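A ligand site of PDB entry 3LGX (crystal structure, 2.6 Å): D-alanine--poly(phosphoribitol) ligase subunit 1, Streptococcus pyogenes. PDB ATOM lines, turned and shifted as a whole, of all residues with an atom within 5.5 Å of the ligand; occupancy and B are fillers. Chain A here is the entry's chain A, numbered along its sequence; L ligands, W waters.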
ATOM      1  N   ARG A  92     -37.863  10.909 -15.637  1.00  0.00           N
ATOM      2  CA  ARG A  92     -37.733  12.242 -15.043  1.00  0.00           C
ATOM      3  C   ARG A  92     -38.622  13.291 -15.752  1.00  0.00           C
ATOM      4  O   ARG A  92     -39.387  14.011 -15.103  1.00  0.00           O
ATOM      5  CB  ARG A  92     -36.245  12.640 -14.976  1.00  0.00           C
ATOM      6  CG  ARG A  92     -35.949  14.109 -14.849  1.00  0.00           C
ATOM      7  CD  ARG A  92     -36.460  14.671 -13.549  1.00  0.00           C
ATOM      8  NE  ARG A  92     -35.535  14.493 -12.422  1.00  0.00           N
ATOM      9  CZ  ARG A  92     -34.711  15.437 -11.961  1.00  0.00           C
ATOM     10  NH1 ARG A  92     -33.918  15.168 -10.919  1.00  0.00           N
ATOM     11  NH2 ARG A  92     -34.661  16.651 -12.532  1.00  0.00           N
ATOM     12  N   PHE A 152     -36.620  22.243 -11.326  1.00  0.00           N
ATOM     13  CA  PHE A 152     -36.797  21.021 -10.594  1.00  0.00           C
ATOM     14  C   PHE A 152     -35.509  20.536  -9.978  1.00  0.00           C
ATOM     15  O   PHE A 152     -34.408  20.541 -10.568  1.00  0.00           O
ATOM     16  CB  PHE A 152     -37.447  19.944 -11.474  1.00  0.00           C
ATOM     17  CG  PHE A 152     -38.937  20.037 -11.513  1.00  0.00           C
ATOM     18  CD1 PHE A 152     -39.724  19.163 -10.759  1.00  0.00           C
ATOM     19  CD2 PHE A 152     -39.568  21.008 -12.308  1.00  0.00           C
ATOM     20  CE1 PHE A 152     -41.107  19.239 -10.781  1.00  0.00           C
ATOM     21  CE2 PHE A 152     -40.956  21.101 -12.347  1.00  0.00           C
ATOM     22  CZ  PHE A 152     -41.728  20.212 -11.566  1.00  0.00           C
ATOM     23  N   THR A 153     -35.647  20.120  -8.739  1.00  0.00           N
ATOM     24  CA  THR A 153     -34.522  19.773  -7.942  1.00  0.00           C
ATOM     25  C   THR A 153     -34.701  18.285  -7.793  1.00  0.00           C
ATOM     26  O   THR A 153     -35.853  17.809  -7.783  1.00  0.00           O
ATOM     27  CB  THR A 153     -34.690  20.486  -6.621  1.00  0.00           C
ATOM     28  OG1 THR A 153     -33.539  21.290  -6.371  1.00  0.00           O
ATOM     29  CG2 THR A 153     -34.985  19.523  -5.475  1.00  0.00           C
ATOM     30  N   SER A 154     -33.604  17.532  -7.708  1.00  0.00           N
ATOM     31  CA  SER A 154     -33.753  16.087  -7.457  1.00  0.00           C
ATOM     32  C   SER A 154     -34.036  15.837  -5.951  1.00  0.00           C
ATOM     33  O   SER A 154     -33.115  15.891  -5.106  1.00  0.00           O
ATOM     34  CB  SER A 154     -32.525  15.309  -7.908  1.00  0.00           C
ATOM     35  OG  SER A 154     -31.577  15.221  -6.847  1.00  0.00           O
ATOM     36  N   THR A 157     -31.543  13.792  -2.800  1.00  0.00           N
ATOM     37  CA  THR A 157     -32.677  13.194  -2.038  1.00  0.00           C
ATOM     38  C   THR A 157     -33.580  12.179  -2.815  1.00  0.00           C
ATOM     39  O   THR A 157     -34.387  11.462  -2.207  1.00  0.00           O
ATOM     40  CB  THR A 157     -33.493  14.305  -1.250  1.00  0.00           C
ATOM     41  OG1 THR A 157     -34.897  13.999  -1.254  1.00  0.00           O
ATOM     42  CG2 THR A 157     -33.262  15.709  -1.848  1.00  0.00           C
ATOM     43  N   PHE A 199     -30.795  23.858 -14.443  1.00  0.00           N
ATOM     44  CA  PHE A 199     -30.058  23.970 -13.205  1.00  0.00           C
ATOM     45  C   PHE A 199     -30.078  25.470 -12.890  1.00  0.00           C
ATOM     46  O   PHE A 199     -29.729  26.298 -13.759  1.00  0.00           O
ATOM     47  CB  PHE A 199     -28.639  23.512 -13.508  1.00  0.00           C
ATOM     48  CG  PHE A 199     -27.686  23.545 -12.355  1.00  0.00           C
ATOM     49  CD1 PHE A 199     -28.141  23.430 -11.052  1.00  0.00           C
ATOM     50  CD2 PHE A 199     -26.311  23.590 -12.594  1.00  0.00           C
ATOM     51  CE1 PHE A 199     -27.236  23.429 -10.015  1.00  0.00           C
ATOM     52  CE2 PHE A 199     -25.392  23.562 -11.535  1.00  0.00           C
ATOM     53  CZ  PHE A 199     -25.866  23.491 -10.271  1.00  0.00           C
ATOM     54  N   ASP A 200     -30.486  25.832 -11.683  1.00  0.00           N
ATOM     55  CA  ASP A 200     -30.632  27.256 -11.383  1.00  0.00           C
ATOM     56  C   ASP A 200     -29.300  28.063 -11.335  1.00  0.00           C
ATOM     57  O   ASP A 200     -29.268  29.286 -11.288  1.00  0.00           O
ATOM     58  CB  ASP A 200     -31.576  27.478 -10.192  1.00  0.00           C
ATOM     59  CG  ASP A 200     -30.859  27.677  -8.881  1.00  0.00           C
ATOM     60  OD1 ASP A 200     -31.377  28.518  -8.115  1.00  0.00           O
ATOM     61  OD2 ASP A 200     -29.833  27.019  -8.586  1.00  0.00           O
ATOM     62  N   PHE A 271     -18.250  30.592  -8.722  1.00  0.00           N
ATOM     63  CA  PHE A 271     -18.608  29.227  -8.353  1.00  0.00           C
ATOM     64  C   PHE A 271     -19.744  29.149  -7.372  1.00  0.00           C
ATOM     65  O   PHE A 271     -19.750  29.874  -6.386  1.00  0.00           O
ATOM     66  CB  PHE A 271     -17.426  28.498  -7.753  1.00  0.00           C
ATOM     67  CG  PHE A 271     -16.299  28.334  -8.685  1.00  0.00           C
ATOM     68  CD1 PHE A 271     -16.434  27.550  -9.821  1.00  0.00           C
ATOM     69  CD2 PHE A 271     -15.069  28.959  -8.430  1.00  0.00           C
ATOM     70  CE1 PHE A 271     -15.364  27.376 -10.697  1.00  0.00           C
ATOM     71  CE2 PHE A 271     -13.999  28.785  -9.305  1.00  0.00           C
ATOM     72  CZ  PHE A 271     -14.155  28.008 -10.434  1.00  0.00           C
ATOM     73  N   ASP A 272     -20.679  28.239  -7.633  1.00  0.00           N
ATOM     74  CA  ASP A 272     -21.793  27.978  -6.720  1.00  0.00           C
ATOM     75  C   ASP A 272     -22.194  26.517  -6.916  1.00  0.00           C
ATOM     76  O   ASP A 272     -21.874  25.924  -7.949  1.00  0.00           O
ATOM     77  CB  ASP A 272     -22.910  28.935  -7.086  1.00  0.00           C
ATOM     78  CG  ASP A 272     -24.136  28.826  -6.211  1.00  0.00           C
ATOM     79  OD1 ASP A 272     -24.211  28.030  -5.244  1.00  0.00           O
ATOM     80  OD2 ASP A 272     -25.069  29.592  -6.513  1.00  0.00           O
ATOM     81  N   GLY A 273     -22.856  25.928  -5.916  1.00  0.00           N
ATOM     82  CA  GLY A 273     -23.504  24.625  -6.099  1.00  0.00           C
ATOM     83  C   GLY A 273     -22.972  23.478  -5.248  1.00  0.00           C
ATOM     84  O   GLY A 273     -23.748  22.622  -4.843  1.00  0.00           O
ATOM     85  N   GLU A 274     -21.669  23.471  -4.975  1.00  0.00           N
ATOM     86  CA  GLU A 274     -21.057  22.493  -4.093  1.00  0.00           C
ATOM     87  C   GLU A 274     -19.859  23.129  -3.424  1.00  0.00           C
ATOM     88  O   GLU A 274     -19.479  24.257  -3.744  1.00  0.00           O
ATOM     89  CB  GLU A 274     -20.646  21.203  -4.837  1.00  0.00           C
ATOM     90  CG  GLU A 274     -19.979  21.454  -6.179  1.00  0.00           C
ATOM     91  CD  GLU A 274     -19.283  20.251  -6.847  1.00  0.00           C
ATOM     92  OE1 GLU A 274     -18.582  20.504  -7.847  1.00  0.00           O
ATOM     93  OE2 GLU A 274     -19.386  19.078  -6.400  1.00  0.00           O
ATOM     94  N   GLU A 275     -19.261  22.427  -2.486  1.00  0.00           N
ATOM     95  CA  GLU A 275     -18.091  22.954  -1.862  1.00  0.00           C
ATOM     96  C   GLU A 275     -17.001  23.313  -2.877  1.00  0.00           C
ATOM     97  O   GLU A 275     -16.605  22.461  -3.682  1.00  0.00           O
ATOM     98  CB  GLU A 275     -17.539  21.986  -0.844  1.00  0.00           C
ATOM     99  CG  GLU A 275     -16.409  22.636  -0.064  1.00  0.00           C
ATOM    100  CD  GLU A 275     -16.448  22.301   1.391  1.00  0.00           C
ATOM    101  OE1 GLU A 275     -17.284  21.495   1.776  1.00  0.00           O
ATOM    102  OE2 GLU A 275     -15.630  22.858   2.150  1.00  0.00           O
ATOM    103  N   LEU A 276     -16.528  24.552  -2.821  1.00  0.00           N
ATOM    104  CA  LEU A 276     -15.292  24.927  -3.476  1.00  0.00           C
ATOM    105  C   LEU A 276     -14.133  24.663  -2.529  1.00  0.00           C
ATOM    106  O   LEU A 276     -14.083  25.147  -1.397  1.00  0.00           O
ATOM    107  CB  LEU A 276     -15.276  26.369  -3.984  1.00  0.00           C
ATOM    108  CG  LEU A 276     -13.970  26.831  -4.661  1.00  0.00           C
ATOM    109  CD1 LEU A 276     -13.918  26.422  -6.110  1.00  0.00           C
ATOM    110  CD2 LEU A 276     -13.804  28.314  -4.541  1.00  0.00           C
ATOM    111  N   ASN A 295     -16.733  32.374  -4.334  1.00  0.00           N
ATOM    112  CA  ASN A 295     -17.535  31.242  -3.867  1.00  0.00           C
ATOM    113  C   ASN A 295     -18.866  31.815  -3.500  1.00  0.00           C
ATOM    114  O   ASN A 295     -18.935  32.831  -2.818  1.00  0.00           O
ATOM    115  CB  ASN A 295     -16.918  30.546  -2.642  1.00  0.00           C
ATOM    116  CG  ASN A 295     -17.534  29.175  -2.381  1.00  0.00           C
ATOM    117  OD1 ASN A 295     -18.173  28.602  -3.250  1.00  0.00           O
ATOM    118  ND2 ASN A 295     -17.315  28.624  -1.205  1.00  0.00           N
ATOM    119  N   ALA A 296     -19.936  31.181  -3.975  1.00  0.00           N
ATOM    120  CA  ALA A 296     -21.280  31.683  -3.741  1.00  0.00           C
ATOM    121  C   ALA A 296     -22.113  30.523  -3.338  1.00  0.00           C
ATOM    122  O   ALA A 296     -21.833  29.396  -3.729  1.00  0.00           O
ATOM    123  CB  ALA A 296     -21.830  32.299  -4.967  1.00  0.00           C
ATOM    124  N   TYR A 297     -23.139  30.792  -2.531  1.00  0.00           N
ATOM    125  CA  TYR A 297     -23.864  29.720  -1.861  1.00  0.00           C
ATOM    126  C   TYR A 297     -25.333  29.963  -1.808  1.00  0.00           C
ATOM    127  O   TYR A 297     -25.791  31.107  -1.704  1.00  0.00           O
ATOM    128  CB  TYR A 297     -23.373  29.532  -0.435  1.00  0.00           C
ATOM    129  CG  TYR A 297     -24.371  28.787   0.449  1.00  0.00           C
ATOM    130  CD1 TYR A 297     -24.388  27.410   0.494  1.00  0.00           C
ATOM    131  CD2 TYR A 297     -25.285  29.492   1.263  1.00  0.00           C
ATOM    132  CE1 TYR A 297     -25.299  26.720   1.315  1.00  0.00           C
ATOM    133  CE2 TYR A 297     -26.171  28.830   2.085  1.00  0.00           C
ATOM    134  CZ  TYR A 297     -26.176  27.446   2.089  1.00  0.00           C
ATOM    135  OH  TYR A 297     -27.073  26.766   2.886  1.00  0.00           O
ATOM    136  N   GLY A 298     -26.057  28.856  -1.863  1.00  0.00           N
ATOM    137  CA  GLY A 298     -27.487  28.833  -1.655  1.00  0.00           C
ATOM    138  C   GLY A 298     -28.141  27.691  -2.392  1.00  0.00           C
ATOM    139  O   GLY A 298     -27.606  27.178  -3.379  1.00  0.00           O
ATOM    140  N   PRO A 299     -29.302  27.280  -1.872  1.00  0.00           N
ATOM    141  CA  PRO A 299     -30.240  26.368  -2.486  1.00  0.00           C
ATOM    142  C   PRO A 299     -31.078  27.110  -3.516  1.00  0.00           C
ATOM    143  O   PRO A 299     -31.197  28.342  -3.475  1.00  0.00           O
ATOM    144  CB  PRO A 299     -31.141  25.998  -1.305  1.00  0.00           C
ATOM    145  CG  PRO A 299     -31.222  27.255  -0.544  1.00  0.00           C
ATOM    146  CD  PRO A 299     -29.771  27.700  -0.549  1.00  0.00           C
ATOM    147  N   THR A 300     -31.683  26.327  -4.401  1.00  0.00           N
ATOM    148  CA  THR A 300     -32.561  26.799  -5.447  1.00  0.00           C
ATOM    149  C   THR A 300     -33.744  27.466  -4.803  1.00  0.00           C
ATOM    150  O   THR A 300     -34.326  28.420  -5.356  1.00  0.00           O
ATOM    151  CB  THR A 300     -33.038  25.596  -6.244  1.00  0.00           C
ATOM    152  OG1 THR A 300     -31.900  24.880  -6.698  1.00  0.00           O
ATOM    153  CG2 THR A 300     -33.890  26.014  -7.473  1.00  0.00           C
ATOM    154  N   GLU A 301     -34.109  26.959  -3.618  1.00  0.00           N
ATOM    155  CA  GLU A 301     -35.267  27.463  -2.901  1.00  0.00           C
ATOM    156  C   GLU A 301     -35.122  28.934  -2.423  1.00  0.00           C
ATOM    157  O   GLU A 301     -36.122  29.570  -2.099  1.00  0.00           O
ATOM    158  CB  GLU A 301     -35.637  26.533  -1.768  1.00  0.00           C
ATOM    159  CG  GLU A 301     -36.074  25.137  -2.246  1.00  0.00           C
ATOM    160  CD  GLU A 301     -34.925  24.161  -2.429  1.00  0.00           C
ATOM    161  OE1 GLU A 301     -33.773  24.619  -2.485  1.00  0.00           O
ATOM    162  OE2 GLU A 301     -35.147  22.930  -2.549  1.00  0.00           O
ATOM    163  N   ILE A 324     -18.242  30.619   2.852  1.00  0.00           N
ATOM    164  CA  ILE A 324     -19.275  30.757   1.814  1.00  0.00           C
ATOM    165  C   ILE A 324     -19.897  32.134   1.721  1.00  0.00           C
ATOM    166  O   ILE A 324     -20.760  32.378   0.859  1.00  0.00           O
ATOM    167  CB  ILE A 324     -20.323  29.640   1.834  1.00  0.00           C
ATOM    168  CG1 ILE A 324     -20.877  29.425   3.249  1.00  0.00           C
ATOM    169  CG2 ILE A 324     -19.683  28.344   1.265  1.00  0.00           C
ATOM    170  CD1 ILE A 324     -22.261  28.762   3.296  1.00  0.00           C
ATOM    171  N   THR A 384     -32.446  25.231   5.035  1.00  0.00           N
ATOM    172  CA  THR A 384     -31.510  24.812   3.984  1.00  0.00           C
ATOM    173  C   THR A 384     -31.068  23.329   4.041  1.00  0.00           C
ATOM    174  O   THR A 384     -30.560  22.775   3.048  1.00  0.00           O
ATOM    175  CB  THR A 384     -30.236  25.687   3.887  1.00  0.00           C
ATOM    176  OG1 THR A 384     -29.440  25.483   5.044  1.00  0.00           O
ATOM    177  CG2 THR A 384     -30.559  27.116   3.755  1.00  0.00           C
ATOM    178  N   ASP A 386     -28.548  22.505   5.537  1.00  0.00           N
ATOM    179  CA  ASP A 386     -27.105  22.611   5.726  1.00  0.00           C
ATOM    180  C   ASP A 386     -26.759  23.018   7.169  1.00  0.00           C
ATOM    181  O   ASP A 386     -27.465  23.818   7.777  1.00  0.00           O
ATOM    182  CB  ASP A 386     -26.543  23.669   4.781  1.00  0.00           C
ATOM    183  CG  ASP A 386     -26.789  23.348   3.306  1.00  0.00           C
ATOM    184  OD1 ASP A 386     -27.297  24.233   2.556  1.00  0.00           O
ATOM    185  OD2 ASP A 386     -26.456  22.219   2.884  1.00  0.00           O
ATOM    186  N   TYR A 398     -19.383  27.010   6.146  1.00  0.00           N
ATOM    187  CA  TYR A 398     -20.122  25.866   5.698  1.00  0.00           C
ATOM    188  C   TYR A 398     -19.600  24.582   6.354  1.00  0.00           C
ATOM    189  O   TYR A 398     -18.405  24.284   6.287  1.00  0.00           O
ATOM    190  CB  TYR A 398     -20.112  25.787   4.144  1.00  0.00           C
ATOM    191  CG  TYR A 398     -20.763  24.536   3.609  1.00  0.00           C
ATOM    192  CD1 TYR A 398     -22.141  24.414   3.588  1.00  0.00           C
ATOM    193  CD2 TYR A 398     -19.998  23.462   3.149  1.00  0.00           C
ATOM    194  CE1 TYR A 398     -22.751  23.248   3.128  1.00  0.00           C
ATOM    195  CE2 TYR A 398     -20.609  22.283   2.683  1.00  0.00           C
ATOM    196  CZ  TYR A 398     -21.992  22.206   2.688  1.00  0.00           C
ATOM    197  OH  TYR A 398     -22.626  21.076   2.225  1.00  0.00           O
ATOM    198  N   ARG A 401     -24.138  18.905   5.009  1.00  0.00           N
ATOM    199  CA  ARG A 401     -25.550  18.600   5.090  1.00  0.00           C
ATOM    200  C   ARG A 401     -25.905  17.870   6.382  1.00  0.00           C
ATOM    201  O   ARG A 401     -25.128  17.053   6.863  1.00  0.00           O
ATOM    202  CB  ARG A 401     -25.979  17.748   3.891  1.00  0.00           C
ATOM    203  CG  ARG A 401     -25.449  18.192   2.549  1.00  0.00           C
ATOM    204  CD  ARG A 401     -26.580  18.263   1.568  1.00  0.00           C
ATOM    205  NE  ARG A 401     -27.424  19.443   1.858  1.00  0.00           N
ATOM    206  CZ  ARG A 401     -28.738  19.425   2.034  1.00  0.00           C
ATOM    207  NH1 ARG A 401     -29.371  20.563   2.278  1.00  0.00           N
ATOM    208  NH2 ARG A 401     -29.434  18.289   1.947  1.00  0.00           N
ATOM    209  N   ASN A 498     -26.130  17.934 -13.182  1.00  0.00           N
ATOM    210  CA  ASN A 498     -25.827  19.351 -13.014  1.00  0.00           C
ATOM    211  C   ASN A 498     -24.360  19.642 -12.811  1.00  0.00           C
ATOM    212  O   ASN A 498     -23.993  20.815 -12.730  1.00  0.00           O
ATOM    213  CB  ASN A 498     -26.675  19.989 -11.907  1.00  0.00           C
ATOM    214  CG  ASN A 498     -28.176  20.006 -12.239  1.00  0.00           C
ATOM    215  OD1 ASN A 498     -28.576  20.031 -13.409  1.00  0.00           O
ATOM    216  ND2 ASN A 498     -29.009  19.995 -11.194  1.00  0.00           N
ATOM    217  N   LYS A 500     -22.156  18.274 -10.199  1.00  0.00           N
ATOM    218  CA  LYS A 500     -21.609  18.188  -8.845  1.00  0.00           C
ATOM    219  C   LYS A 500     -21.081  16.774  -8.556  1.00  0.00           C
ATOM    220  O   LYS A 500     -21.522  15.820  -9.223  1.00  0.00           O
ATOM    221  CB  LYS A 500     -22.686  18.494  -7.827  1.00  0.00           C
ATOM    222  CG  LYS A 500     -23.453  19.733  -8.083  1.00  0.00           C
ATOM    223  CD  LYS A 500     -24.596  19.799  -7.071  1.00  0.00           C
ATOM    224  CE  LYS A 500     -25.396  21.088  -7.186  1.00  0.00           C
ATOM    225  NZ  LYS A 500     -25.945  21.370  -5.811  1.00  0.00           N
HETATM  226  P1  LIG L   1     -29.935  19.691  -7.929  1.00  0.00           P
HETATM  227  O1  LIG L   1     -31.089  20.666  -7.810  1.00  0.00           O
HETATM  228  O2  LIG L   1     -30.182  18.629  -8.971  1.00  0.00           O
HETATM  229  O3  LIG L   1     -28.573  20.355  -7.955  1.00  0.00           O
HETATM  230  P2  LIG L   1     -29.862  19.677  -5.107  1.00  0.00           P
HETATM  231  O4  LIG L   1     -28.419  19.669  -4.672  1.00  0.00           O
HETATM  232  O5  LIG L   1     -30.975  19.045  -4.309  1.00  0.00           O
HETATM  233  O6  LIG L   1     -29.921  18.914  -6.518  1.00  0.00           O
HETATM  234  P3  LIG L   1     -29.534  22.581  -5.207  1.00  0.00           P
HETATM  235  O7  LIG L   1     -30.518  23.681  -5.006  1.00  0.00           O
HETATM  236  O8  LIG L   1     -28.565  22.682  -6.339  1.00  0.00           O
HETATM  237  O9  LIG L   1     -30.370  21.205  -5.375  1.00  0.00           O
HETATM  238  O10 LIG L   1     -28.669  22.335  -3.863  1.00  0.00           O
HETATM  239  C1  LIG L   1     -28.240  23.410  -3.027  1.00  0.00           C
HETATM  240  C2  LIG L   1     -27.236  22.815  -2.062  1.00  0.00           C
HETATM  241  O11 LIG L   1     -25.922  22.773  -2.621  1.00  0.00           O
HETATM  242  C3  LIG L   1     -27.080  23.563  -0.751  1.00  0.00           C
HETATM  243  O12 LIG L   1     -27.979  22.991   0.187  1.00  0.00           O
HETATM  244  C4  LIG L   1     -25.683  23.206  -0.311  1.00  0.00           C
HETATM  245  O13 LIG L   1     -25.729  21.922   0.307  1.00  0.00           O
HETATM  246  C5  LIG L   1     -24.940  23.008  -1.609  1.00  0.00           C
HETATM  247  N1  LIG L   1     -24.137  24.178  -2.005  1.00  0.00           N
HETATM  248  C6  LIG L   1     -24.534  25.126  -2.843  1.00  0.00           C
HETATM  249  N2  LIG L   1     -23.553  26.056  -2.963  1.00  0.00           N
HETATM  250  C7  LIG L   1     -22.510  25.694  -2.194  1.00  0.00           C
HETATM  251  C8  LIG L   1     -21.175  26.195  -1.890  1.00  0.00           C
HETATM  252  N3  LIG L   1     -20.720  27.351  -2.434  1.00  0.00           N
HETATM  253  N4  LIG L   1     -20.394  25.509  -1.031  1.00  0.00           N
HETATM  254  C9  LIG L   1     -20.825  24.394  -0.449  1.00  0.00           C
HETATM  255  N5  LIG L   1     -22.034  23.875  -0.701  1.00  0.00           N
HETATM  256  C10 LIG L   1     -22.916  24.464  -1.556  1.00  0.00           C
HETATM  257  O   HOH W   1     -33.701  19.836  -2.359  1.00  0.00           O
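O7 of the ligand is in hydrogen-bond range of N of Thr 300. An oxygen (O7) of the ligand is in hydrogen-bond range of the side-chain hydroxyl (OG1) of Thr 300 (2.5 Å). N3 of the ligand sits at hydrogen-bond distance from O of Ala 296 (2.7 Å). OD2 of Asp 386 is in hydrogen-bond range of O13 of the ligand, 2.7 Å away. An oxygen (O2) of the ligand is in hydrogen-bond range of the side-chain amide nitrogen (ND2) of Asn 498. OG1 of Thr 153 is in hydrogen-bond range of O1 of the ligand (2.9 Å). OD1 of Asn 295 lies within hydrogen-bond range of N3 of the ligand, 3.0 Å away. The side-chain amino group (NZ) of Lys 500 is in salt-bridge range of an oxygen (O8) of the ligand. N of Gly 273 lies within hydrogen-bond range of N2 of the ligand. The guanidinium group of Arg 401 is in hydrogen-bond range of an oxygen (O13) of the ligand, at 3.4 Å.
Water W1 lies within hydrogen-bond range of OE2 of Glu 301 (3.4 Å) and O5 of the ligand (3.4 Å).
The backbone NH (N) of Ala 296 sits at hydrogen-bond distance from the backbone carbonyl oxygen (O) of Phe 271 (2.7 Å). The guanidinium group (NE) of Arg 401 lies within salt-bridge range of the side-chain carboxylate (OD2) of Asp 386, at 3.1 Å. OD1 of Asp 386 lies within hydrogen-bond range of OH of Tyr 297 (2.6 Å). OG1 of Thr 384 sits close to N of Asp 386 (3.1 Å). The side-chain amino group (NZ) of Lys 500 is in hydrogen-bond range of the backbone carbonyl oxygen (O) of Gly 273 (2.7 Å). The backbone carbonyl oxygen of Thr 384 is in hydrogen-bond range of the guanidinium group of Arg 401 (2.6 Å). The side-chain hydroxyl (OH) of Tyr 297 is in hydrogen-bond range of the side-chain hydroxyl (OG1) of Thr 384.
A nitrogen (N2) of the ligand sits close to the side-chain carboxylate of Asp 272 (3.1 Å). A nitrogen (N4) of the ligand sits close to the backbone carbonyl oxygen (O) of Glu 274 (3.1 Å). Ser 154 touches the ligand. CE1 of Phe 199 touches O3 of the ligand, at 3.9 Å. Glu 275 touches the ligand. CD1 of Tyr 297 touches C7 of the ligand (3.7 Å). Gly 298 touches the ligand (O to C6, 3.7 Å). CA of Pro 299 touches C1 of the ligand (3.6 Å). Ile 324 touches the ligand (CG2 to N4, 3.7 Å). Thr 384 touches the ligand. Tyr 398 touches the ligand. Hydrophobic or aromatic side chains within 4 Å of the ligand: Phe 199, Tyr 297, Ile 324 and Tyr 398. Within 4 Å of the ligand: Thr 153, Ser 154, Phe 199, Asp 272, Gly 273, Glu 274, Glu 275, Asn 295, Ala 296, Tyr 297, Gly 298, Pro 299, Thr 300, Ile 324, Thr 384, Asp 386, Tyr 398, Arg 401, Asn 498 and Lys 500. The nearest printed residue that does not touch the ligand is Glu 301 (4.2 Å).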
